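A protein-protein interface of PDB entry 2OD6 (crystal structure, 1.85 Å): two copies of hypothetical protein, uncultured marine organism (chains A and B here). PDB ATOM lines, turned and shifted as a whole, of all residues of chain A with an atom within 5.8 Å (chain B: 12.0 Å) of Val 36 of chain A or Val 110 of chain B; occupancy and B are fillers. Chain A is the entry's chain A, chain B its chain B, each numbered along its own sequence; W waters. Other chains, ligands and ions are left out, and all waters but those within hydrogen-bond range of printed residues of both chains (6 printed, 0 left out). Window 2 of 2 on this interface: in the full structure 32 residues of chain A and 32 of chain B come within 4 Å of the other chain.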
ATOM      1  N   THR A  31     -10.402  25.881  -9.615  1.00  0.00           N
ATOM      2  CA  THR A  31      -9.762  24.560  -9.627  1.00  0.00           C
ATOM      3  C   THR A  31     -10.107  23.748 -10.880  1.00  0.00           C
ATOM      4  O   THR A  31      -9.579  22.640 -11.107  1.00  0.00           O
ATOM      5  CB  THR A  31     -10.126  23.776  -8.360  1.00  0.00           C
ATOM      6  OG1 THR A  31     -11.539  23.555  -8.301  1.00  0.00           O
ATOM      7  CG2 THR A  31      -9.683  24.559  -7.112  1.00  0.00           C
ATOM      8  N   ALA A  32     -10.924  24.334 -11.750  1.00  0.00           N
ATOM      9  CA  ALA A  32     -11.391  23.656 -12.965  1.00  0.00           C
ATOM     10  C   ALA A  32     -10.266  23.161 -13.884  1.00  0.00           C
ATOM     11  O   ALA A  32     -10.397  22.118 -14.511  1.00  0.00           O
ATOM     12  CB  ALA A  32     -12.334  24.578 -13.725  1.00  0.00           C
ATOM     13  N   PRO A  33      -9.169  23.919 -13.995  1.00  0.00           N
ATOM     14  CA  PRO A  33      -8.057  23.426 -14.810  1.00  0.00           C
ATOM     15  C   PRO A  33      -7.511  22.048 -14.412  1.00  0.00           C
ATOM     16  O   PRO A  33      -6.975  21.342 -15.272  1.00  0.00           O
ATOM     17  CB  PRO A  33      -6.976  24.507 -14.636  1.00  0.00           C
ATOM     18  CG  PRO A  33      -7.752  25.748 -14.359  1.00  0.00           C
ATOM     19  CD  PRO A  33      -8.915  25.281 -13.503  1.00  0.00           C
ATOM     20  N   VAL A  34      -7.624  21.691 -13.135  1.00  0.00           N
ATOM     21  CA  VAL A  34      -7.269  20.374 -12.651  1.00  0.00           C
ATOM     22  C   VAL A  34      -8.415  19.391 -12.925  1.00  0.00           C
ATOM     23  O   VAL A  34      -8.254  18.458 -13.705  1.00  0.00           O
ATOM     24  CB  VAL A  34      -6.900  20.416 -11.138  1.00  0.00           C
ATOM     25  CG1 VAL A  34      -6.569  19.005 -10.605  1.00  0.00           C
ATOM     26  CG2 VAL A  34      -5.696  21.358 -10.910  1.00  0.00           C
ATOM     27  N   TRP A  35      -9.580  19.607 -12.313  1.00  0.00           N
ATOM     28  CA  TRP A  35     -10.585  18.553 -12.260  1.00  0.00           C
ATOM     29  C   TRP A  35     -11.309  18.312 -13.576  1.00  0.00           C
ATOM     30  O   TRP A  35     -11.663  17.168 -13.870  1.00  0.00           O
ATOM     31  CB  TRP A  35     -11.558  18.731 -11.091  1.00  0.00           C
ATOM     32  CG  TRP A  35     -12.376  19.969 -11.083  1.00  0.00           C
ATOM     33  CD1 TRP A  35     -12.120  21.106 -10.371  1.00  0.00           C
ATOM     34  CD2 TRP A  35     -13.605  20.198 -11.779  1.00  0.00           C
ATOM     35  NE1 TRP A  35     -13.082  22.039 -10.610  1.00  0.00           N
ATOM     36  CE2 TRP A  35     -14.016  21.511 -11.465  1.00  0.00           C
ATOM     37  CE3 TRP A  35     -14.400  19.421 -12.637  1.00  0.00           C
ATOM     38  CZ2 TRP A  35     -15.188  22.076 -11.983  1.00  0.00           C
ATOM     39  CZ3 TRP A  35     -15.572  19.986 -13.170  1.00  0.00           C
ATOM     40  CH2 TRP A  35     -15.951  21.304 -12.841  1.00  0.00           C
ATOM     41  N   VAL A  36     -11.485  19.346 -14.404  1.00  0.00           N
ATOM     42  CA  VAL A  36     -12.262  19.181 -15.642  1.00  0.00           C
ATOM     43  C   VAL A  36     -11.518  18.250 -16.584  1.00  0.00           C
ATOM     44  O   VAL A  36     -12.095  17.289 -17.115  1.00  0.00           O
ATOM     45  CB  VAL A  36     -12.610  20.533 -16.372  1.00  0.00           C
ATOM     46  CG1 VAL A  36     -13.427  20.250 -17.614  1.00  0.00           C
ATOM     47  CG2 VAL A  36     -13.388  21.476 -15.484  1.00  0.00           C
ATOM     48  N   LYS A  37     -10.223  18.502 -16.740  1.00  0.00           N
ATOM     49  CA  LYS A  37      -9.381  17.684 -17.575  1.00  0.00           C
ATOM     50  C   LYS A  37      -9.460  16.232 -17.108  1.00  0.00           C
ATOM     51  O   LYS A  37      -9.553  15.315 -17.922  1.00  0.00           O
ATOM     52  CB  LYS A  37      -7.940  18.198 -17.476  1.00  0.00           C
ATOM     53  CG  LYS A  37      -7.020  17.718 -18.512  1.00  0.00           C
ATOM     54  CD  LYS A  37      -5.632  18.366 -18.377  1.00  0.00           C
ATOM     55  CE  LYS A  37      -4.802  17.780 -17.230  1.00  0.00           C
ATOM     56  NZ  LYS A  37      -5.040  18.485 -15.925  1.00  0.00           N
ATOM     57  N   GLU A  38      -9.408  16.027 -15.795  1.00  0.00           N
ATOM     58  CA  GLU A  38      -9.383  14.667 -15.257  1.00  0.00           C
ATOM     59  C   GLU A  38     -10.675  13.930 -15.509  1.00  0.00           C
ATOM     60  O   GLU A  38     -10.667  12.765 -15.913  1.00  0.00           O
ATOM     61  CB  GLU A  38      -9.071  14.688 -13.763  1.00  0.00           C
ATOM     62  CG  GLU A  38      -7.677  15.146 -13.460  1.00  0.00           C
ATOM     63  CD  GLU A  38      -6.585  14.170 -13.896  1.00  0.00           C
ATOM     64  OE1 GLU A  38      -6.870  13.006 -14.232  1.00  0.00           O
ATOM     65  OE2 GLU A  38      -5.417  14.579 -13.880  1.00  0.00           O
ATOM     66  N   MET A  39     -11.788  14.611 -15.276  1.00  0.00           N
ATOM     67  CA  MET A  39     -13.111  14.007 -15.462  1.00  0.00           C
ATOM     68  C   MET A  39     -13.447  13.719 -16.935  1.00  0.00           C
ATOM     69  O   MET A  39     -14.023  12.677 -17.268  1.00  0.00           O
ATOM     70  CB  MET A  39     -14.198  14.891 -14.810  1.00  0.00           C
ATOM     71  CG  MET A  39     -14.081  14.954 -13.344  1.00  0.00           C
ATOM     72  SD  MET A  39     -15.560  15.839 -12.437  1.00  0.00           S
ATOM     73  CE  MET A  39     -16.904  14.384 -12.267  1.00  0.00           C
ATOM     74  N   LYS A  40     -13.066  14.624 -17.822  1.00  0.00           N
ATOM     75  CA  LYS A  40     -13.316  14.416 -19.219  1.00  0.00           C
ATOM     76  C   LYS A  40     -12.488  13.286 -19.748  1.00  0.00           C
ATOM     77  O   LYS A  40     -12.965  12.531 -20.599  1.00  0.00           O
ATOM     78  CB  LYS A  40     -13.084  15.682 -20.033  1.00  0.00           C
ATOM     79  CG  LYS A  40     -14.122  16.753 -19.766  1.00  0.00           C
ATOM     80  CD  LYS A  40     -14.143  17.749 -20.895  1.00  0.00           C
ATOM     81  CE  LYS A  40     -15.321  18.705 -20.745  1.00  0.00           C
ATOM     82  NZ  LYS A  40     -15.126  19.833 -21.703  1.00  0.00           N
ATOM     83  N   SER A  41     -11.258  13.122 -19.237  1.00  0.00           N
ATOM     84  CA  SER A  41     -10.415  12.005 -19.673  1.00  0.00           C
ATOM     85  C   SER A  41     -11.017  10.675 -19.229  1.00  0.00           C
ATOM     86  O   SER A  41     -10.614   9.631 -19.729  1.00  0.00           O
ATOM     87  CB  SER A  41      -8.997  12.123 -19.116  1.00  0.00           C
ATOM     88  OG  SER A  41      -8.989  11.803 -17.724  1.00  0.00           O
ATOM     89  N   LEU A  44     -16.555  12.194 -18.673  1.00  0.00           N
ATOM     90  CA  LEU A  44     -17.418  13.359 -18.480  1.00  0.00           C
ATOM     91  C   LEU A  44     -17.570  14.056 -19.818  1.00  0.00           C
ATOM     92  O   LEU A  44     -16.584  14.389 -20.469  1.00  0.00           O
ATOM     93  CB  LEU A  44     -16.830  14.358 -17.464  1.00  0.00           C
ATOM     94  CG  LEU A  44     -17.728  15.553 -17.049  1.00  0.00           C
ATOM     95  CD1 LEU A  44     -18.879  15.142 -16.167  1.00  0.00           C
ATOM     96  CD2 LEU A  44     -16.892  16.594 -16.351  1.00  0.00           C
ATOM     97  N   LEU A  45     -18.817  14.253 -20.240  1.00  0.00           N
ATOM     98  CA  LEU A  45     -19.084  14.962 -21.500  1.00  0.00           C
ATOM     99  C   LEU A  45     -19.220  16.482 -21.264  1.00  0.00           C
ATOM    100  O   LEU A  45     -18.717  17.285 -22.060  1.00  0.00           O
ATOM    101  CB  LEU A  45     -20.328  14.390 -22.204  1.00  0.00           C
ATOM    102  CG  LEU A  45     -20.330  12.998 -22.855  1.00  0.00           C
ATOM    103  CD1 LEU A  45     -21.793  12.680 -23.286  1.00  0.00           C
ATOM    104  CD2 LEU A  45     -19.341  12.835 -24.027  1.00  0.00           C
ATOM    105  N   LYS A  46     -19.846  16.865 -20.152  1.00  0.00           N
ATOM    106  CA  LYS A  46     -20.153  18.250 -19.874  1.00  0.00           C
ATOM    107  C   LYS A  46     -20.394  18.425 -18.395  1.00  0.00           C
ATOM    108  O   LYS A  46     -20.934  17.514 -17.711  1.00  0.00           O
ATOM    109  CB  LYS A  46     -21.390  18.712 -20.670  1.00  0.00           C
ATOM    110  CG  LYS A  46     -21.711  20.190 -20.564  1.00  0.00           C
ATOM    111  CD  LYS A  46     -22.993  20.561 -21.333  1.00  0.00           C
ATOM    112  CE  LYS A  46     -23.702  21.786 -20.707  1.00  0.00           C
ATOM    113  NZ  LYS A  46     -24.838  22.184 -21.554  1.00  0.00           N
ATOM    114  N   PHE A  47     -19.975  19.596 -17.895  1.00  0.00           N
ATOM    115  CA  PHE A  47     -20.328  20.054 -16.544  1.00  0.00           C
ATOM    116  C   PHE A  47     -21.035  21.431 -16.611  1.00  0.00           C
ATOM    117  O   PHE A  47     -20.724  22.236 -17.480  1.00  0.00           O
ATOM    118  CB  PHE A  47     -19.077  20.192 -15.700  1.00  0.00           C
ATOM    119  CG  PHE A  47     -19.302  20.888 -14.390  1.00  0.00           C
ATOM    120  CD1 PHE A  47     -19.665  20.169 -13.284  1.00  0.00           C
ATOM    121  CD2 PHE A  47     -19.110  22.278 -14.262  1.00  0.00           C
ATOM    122  CE1 PHE A  47     -19.871  20.799 -12.069  1.00  0.00           C
ATOM    123  CE2 PHE A  47     -19.311  22.921 -13.044  1.00  0.00           C
ATOM    124  CZ  PHE A  47     -19.672  22.173 -11.945  1.00  0.00           C
ATOM    125  N   SER A  48     -21.967  21.702 -15.679  1.00  0.00           N
ATOM    126  CA  SER A  48     -22.574  23.059 -15.564  1.00  0.00           C
ATOM    127  C   SER A  48     -22.898  23.338 -14.160  1.00  0.00           C
ATOM    128  O   SER A  48     -23.131  22.398 -13.433  1.00  0.00           O
ATOM    129  CB  SER A  48     -23.787  23.263 -16.497  1.00  0.00           C
ATOM    130  OG  SER A  48     -24.951  22.578 -16.072  1.00  0.00           O
ATOM    131  N   LYS B   6     -27.557  32.482 -20.120  1.00  0.00           N
ATOM    132  CA  LYS B   6     -28.390  31.362 -20.474  1.00  0.00           C
ATOM    133  C   LYS B   6     -29.226  30.966 -19.264  1.00  0.00           C
ATOM    134  O   LYS B   6     -28.875  31.244 -18.090  1.00  0.00           O
ATOM    135  CB  LYS B   6     -27.590  30.154 -21.026  1.00  0.00           C
ATOM    136  CG  LYS B   6     -26.844  30.415 -22.324  1.00  0.00           C
ATOM    137  CD  LYS B   6     -25.858  29.304 -22.630  1.00  0.00           C
ATOM    138  CE  LYS B   6     -26.494  28.016 -22.977  1.00  0.00           C
ATOM    139  NZ  LYS B   6     -25.437  26.951 -23.314  1.00  0.00           N
ATOM    140  N   THR B   8     -31.616  27.693 -17.577  1.00  0.00           N
ATOM    141  CA  THR B   8     -31.916  26.279 -17.566  1.00  0.00           C
ATOM    142  C   THR B   8     -32.902  26.002 -16.427  1.00  0.00           C
ATOM    143  O   THR B   8     -32.791  26.593 -15.373  1.00  0.00           O
ATOM    144  CB  THR B   8     -30.628  25.410 -17.424  1.00  0.00           C
ATOM    145  OG1 THR B   8     -29.703  25.696 -18.497  1.00  0.00           O
ATOM    146  CG2 THR B   8     -30.983  23.896 -17.376  1.00  0.00           C
ATOM    147  N   LYS B  46     -31.908  22.372 -25.853  1.00  0.00           N
ATOM    148  CA  LYS B  46     -31.860  20.958 -25.580  1.00  0.00           C
ATOM    149  C   LYS B  46     -32.868  20.610 -24.498  1.00  0.00           C
ATOM    150  O   LYS B  46     -33.084  21.414 -23.568  1.00  0.00           O
ATOM    151  CB  LYS B  46     -30.454  20.583 -25.123  1.00  0.00           C
ATOM    152  CG  LYS B  46     -30.311  19.134 -24.683  1.00  0.00           C
ATOM    153  CD  LYS B  46     -28.906  18.829 -24.237  1.00  0.00           C
ATOM    154  CE  LYS B  46     -28.838  17.425 -23.709  1.00  0.00           C
ATOM    155  NZ  LYS B  46     -27.525  17.219 -23.047  1.00  0.00           N
ATOM    156  N   GLU B  66     -32.952  23.579 -21.464  1.00  0.00           N
ATOM    157  CA  GLU B  66     -31.840  24.494 -21.684  1.00  0.00           C
ATOM    158  C   GLU B  66     -32.228  25.508 -22.744  1.00  0.00           C
ATOM    159  O   GLU B  66     -32.459  25.141 -23.874  1.00  0.00           O
ATOM    160  CB  GLU B  66     -30.634  23.726 -22.157  1.00  0.00           C
ATOM    161  CG  GLU B  66     -30.020  22.889 -21.042  1.00  0.00           C
ATOM    162  CD  GLU B  66     -28.857  22.039 -21.510  1.00  0.00           C
ATOM    163  OE1 GLU B  66     -27.955  22.595 -22.172  1.00  0.00           O
ATOM    164  OE2 GLU B  66     -28.848  20.833 -21.197  1.00  0.00           O
ATOM    165  N   LEU B 105     -30.080  30.449 -13.660  1.00  0.00           N
ATOM    166  CA  LEU B 105     -29.136  31.087 -14.582  1.00  0.00           C
ATOM    167  C   LEU B 105     -27.899  30.215 -14.717  1.00  0.00           C
ATOM    168  O   LEU B 105     -27.337  29.737 -13.738  1.00  0.00           O
ATOM    169  CB  LEU B 105     -28.733  32.466 -14.020  1.00  0.00           C
ATOM    170  CG  LEU B 105     -29.836  33.522 -13.932  1.00  0.00           C
ATOM    171  CD1 LEU B 105     -29.479  34.563 -12.884  1.00  0.00           C
ATOM    172  CD2 LEU B 105     -30.064  34.149 -15.311  1.00  0.00           C
ATOM    173  N   VAL B 106     -27.417  30.013 -15.930  1.00  0.00           N
ATOM    174  CA  VAL B 106     -26.194  29.270 -16.081  1.00  0.00           C
ATOM    175  C   VAL B 106     -24.958  30.118 -15.655  1.00  0.00           C
ATOM    176  O   VAL B 106     -24.748  31.213 -16.211  1.00  0.00           O
ATOM    177  CB  VAL B 106     -26.022  28.788 -17.515  1.00  0.00           C
ATOM    178  CG1 VAL B 106     -24.750  28.018 -17.605  1.00  0.00           C
ATOM    179  CG2 VAL B 106     -27.290  27.949 -17.910  1.00  0.00           C
ATOM    180  N   VAL B 107     -24.226  29.627 -14.642  1.00  0.00           N
ATOM    181  CA  VAL B 107     -23.043  30.299 -14.016  1.00  0.00           C
ATOM    182  C   VAL B 107     -21.750  29.882 -14.730  1.00  0.00           C
ATOM    183  O   VAL B 107     -20.902  30.706 -15.043  1.00  0.00           O
ATOM    184  CB  VAL B 107     -23.013  30.024 -12.484  1.00  0.00           C
ATOM    185  CG1 VAL B 107     -21.732  30.533 -11.792  1.00  0.00           C
ATOM    186  CG2 VAL B 107     -24.195  30.678 -11.844  1.00  0.00           C
ATOM    187  N   MET B 108     -21.592  28.582 -14.933  1.00  0.00           N
ATOM    188  CA  MET B 108     -20.460  28.022 -15.637  1.00  0.00           C
ATOM    189  C   MET B 108     -20.924  26.839 -16.465  1.00  0.00           C
ATOM    190  O   MET B 108     -21.850  26.135 -16.095  1.00  0.00           O
ATOM    191  CB  MET B 108     -19.360  27.568 -14.659  1.00  0.00           C
ATOM    192  CG  MET B 108     -18.481  26.438 -15.211  1.00  0.00           C
ATOM    193  SD  MET B 108     -16.911  26.061 -14.204  1.00  0.00           S
ATOM    194  CE  MET B 108     -17.549  26.566 -12.440  1.00  0.00           C
ATOM    195  N   GLU B 109     -20.274  26.635 -17.599  1.00  0.00           N
ATOM    196  CA  GLU B 109     -20.400  25.391 -18.333  1.00  0.00           C
ATOM    197  C   GLU B 109     -19.063  25.052 -19.000  1.00  0.00           C
ATOM    198  O   GLU B 109     -18.382  25.939 -19.571  1.00  0.00           O
ATOM    199  CB  GLU B 109     -21.542  25.407 -19.368  1.00  0.00           C
ATOM    200  CG  GLU B 109     -21.466  26.500 -20.380  1.00  0.00           C
ATOM    201  CD  GLU B 109     -22.745  26.695 -21.173  1.00  0.00           C
ATOM    202  OE1 GLU B 109     -23.526  25.755 -21.333  1.00  0.00           O
ATOM    203  OE2 GLU B 109     -22.922  27.818 -21.664  1.00  0.00           O
ATOM    204  N   VAL B 110     -18.662  23.788 -18.883  1.00  0.00           N
ATOM    205  CA  VAL B 110     -17.468  23.271 -19.621  1.00  0.00           C
ATOM    206  C   VAL B 110     -17.759  21.984 -20.351  1.00  0.00           C
ATOM    207  O   VAL B 110     -18.613  21.191 -19.955  1.00  0.00           O
ATOM    208  CB  VAL B 110     -16.294  22.952 -18.707  1.00  0.00           C
ATOM    209  CG1 VAL B 110     -14.971  23.311 -19.404  1.00  0.00           C
ATOM    210  CG2 VAL B 110     -16.390  23.707 -17.428  1.00  0.00           C
ATOM    211  OXT VAL B 110     -17.113  21.712 -21.367  1.00  0.00           O
HETATM  212  O   HOH W   1     -25.540  24.629 -19.974  1.00  0.00           O
HETATM  213  O   HOH W   2     -26.379  19.693 -21.939  1.00  0.00           O
HETATM  214  O   HOH W   3     -27.332  24.351 -17.728  1.00  0.00           O
HETATM  215  O   HOH W   4     -23.978  23.893 -23.373  1.00  0.00           O
HETATM  216  O   HOH W   5     -18.463  19.893 -22.721  1.00  0.00           O
HETATM  217  O   HOH W   6     -26.749  21.935 -24.453  1.00  0.00           O
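The side-chain amino group of Lys 46 of chain A is in salt-bridge range of the side-chain carboxylate of Glu 66 of chain B, 3.2 Å away.
NZ of Lys 46 of chain A is in salt-bridge range of OE1 of Glu 109 of chain B (3.8 Å).
The chain-end carboxylate (OXT) of Val 110 of chain B lies within salt-bridge range of the side-chain amino group (NZ) of Lys 40 of chain A, at 2.8 Å.
The backbone carbonyl oxygen of Phe 47 of chain A is in hydrogen-bond range of the backbone NH of Val 110 of chain B, 2.9 Å away.
The backbone carbonyl oxygen (O) of Lys 46 of chain B is in hydrogen-bond range of the backbone NH (N) of Glu 66 of chain B (3.0 Å).
The side-chain carboxylate of Glu 109 of chain B is in salt-bridge range of the side-chain amino group of Lys 6 of chain B (3.0 Å).
Among the printed residues, pairs that only touch across the chains: Ser 48 of chain A with Met 108 of chain B (3.2 Å), Phe 47 of chain A with Glu 109 of chain B (3.3 Å), Lys 46 of chain A with Val 110 of chain B (3.3 Å) and Val 36 of chain A with Val 110 of chain B (3.9 Å).
Of chain A, only Val 36, Lys 40, Lys 46 and Phe 47 come within 4 Å of Val 110 of chain B.
Pro 33 of chain A touches none of the printed residues of chain B.
No residue of chain B comes within 4 Å of Val 34 of chain A.
No residue of chain B comes within 4 Å of Glu 38 of chain A.
No residue of chain B comes within 4 Å of Met 39 of chain A.
Leu 44 of chain A touches none of the printed residues of chain B.
Lys 46 of chain A touches just these residues of chain B: Glu 66 (3.2 Å), Glu 109 (3.8 Å) and Val 110 (3.3 Å).
Of chain B, only Glu 109 (3.3 Å) and Val 110 (2.9 Å) come within 4 Å of Phe 47 of chain A.
Of the printed residues of chain B, Ser 48 of chain A touches Met 108.
Of the printed residues of chain A, Glu 66 of chain B touches Lys 46 (3.2 Å).
Of the printed residues of chain A, Met 108 of chain B touches Ser 48.
Of the printed residues of chain A, Glu 109 of chain B touches Lys 46 (3.8 Å) and Phe 47 (3.3 Å).
Leu 45 of chain A touches none of the printed residues of chain B.
The nearest printed residue of chain B that does not touch Val 36 of chain A is Met 108 of chain B (5.9 Å).
The nearest residue of chain A that does not touch Val 110 of chain B is Leu 45 of chain A (4.4 Å).
The nearest printed residue of chain A that does not touch Met 108 of chain B is Phe 47 of chain A (4.1 Å).
Hydrophobic or aromatic side chains of chain B within 4 Å of the printed part of chain A: Val 110.
Printed residues of chain A that touch a printed residue of chain B: Val 36, Lys 40, Lys 46, Phe 47 and Ser 48.
Hydrophobic or aromatic side chains of chain A within 4 Å of the printed part of chain B: Val 36.
Among the printed residues, Asp or Glu carboxylates within 4 Å of a Lys or Arg side-chain nitrogen of the other chain: Lys 46 of chain A with Glu 66 of chain B (3.2 Å) and Lys 46 of chain A with Glu 109 of chain B (3.8 Å).
1 position is printed for both chains.
Of the 8 pairs that touch across the chains among the printed residues, none has its exchanged pair printed and touching as well.
Water W5 lies within hydrogen-bond range of OXT of Val 110 of chain B (2.6 Å), O of Leu 45 of chain A (2.7 Å) and NZ of Lys 40 of chain A (3.5 Å).
Water W4 lies within hydrogen-bond range of NZ of Lys 46 of chain A (2.6 Å), OE1 of Glu 109 of chain B (2.8 Å) and NZ of Lys 6 of chain B (3.4 Å).
Water W6 lies within hydrogen-bond range of the side-chain carboxylate of Glu 66 of chain B and the side-chain amino group of Lys 46 of chain A.
Water W1 lies within hydrogen-bond range of OE1 of Glu 109 of chain B and NZ of Lys 46 of chain A.
Water W2 lies within hydrogen-bond range of the side-chain carboxylate (OE2) of Glu 66 of chain B (2.8 Å), the side-chain amino group (NZ) of Lys 46 of chain B (2.9 Å) and the side-chain amino group (NZ) of Lys 46 of chain A (3.0 Å).
Water W3 lies within hydrogen-bond range of OG1 of Thr 8 of chain B (2.8 Å) and OG of Ser 48 of chain A (3.4 Å).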
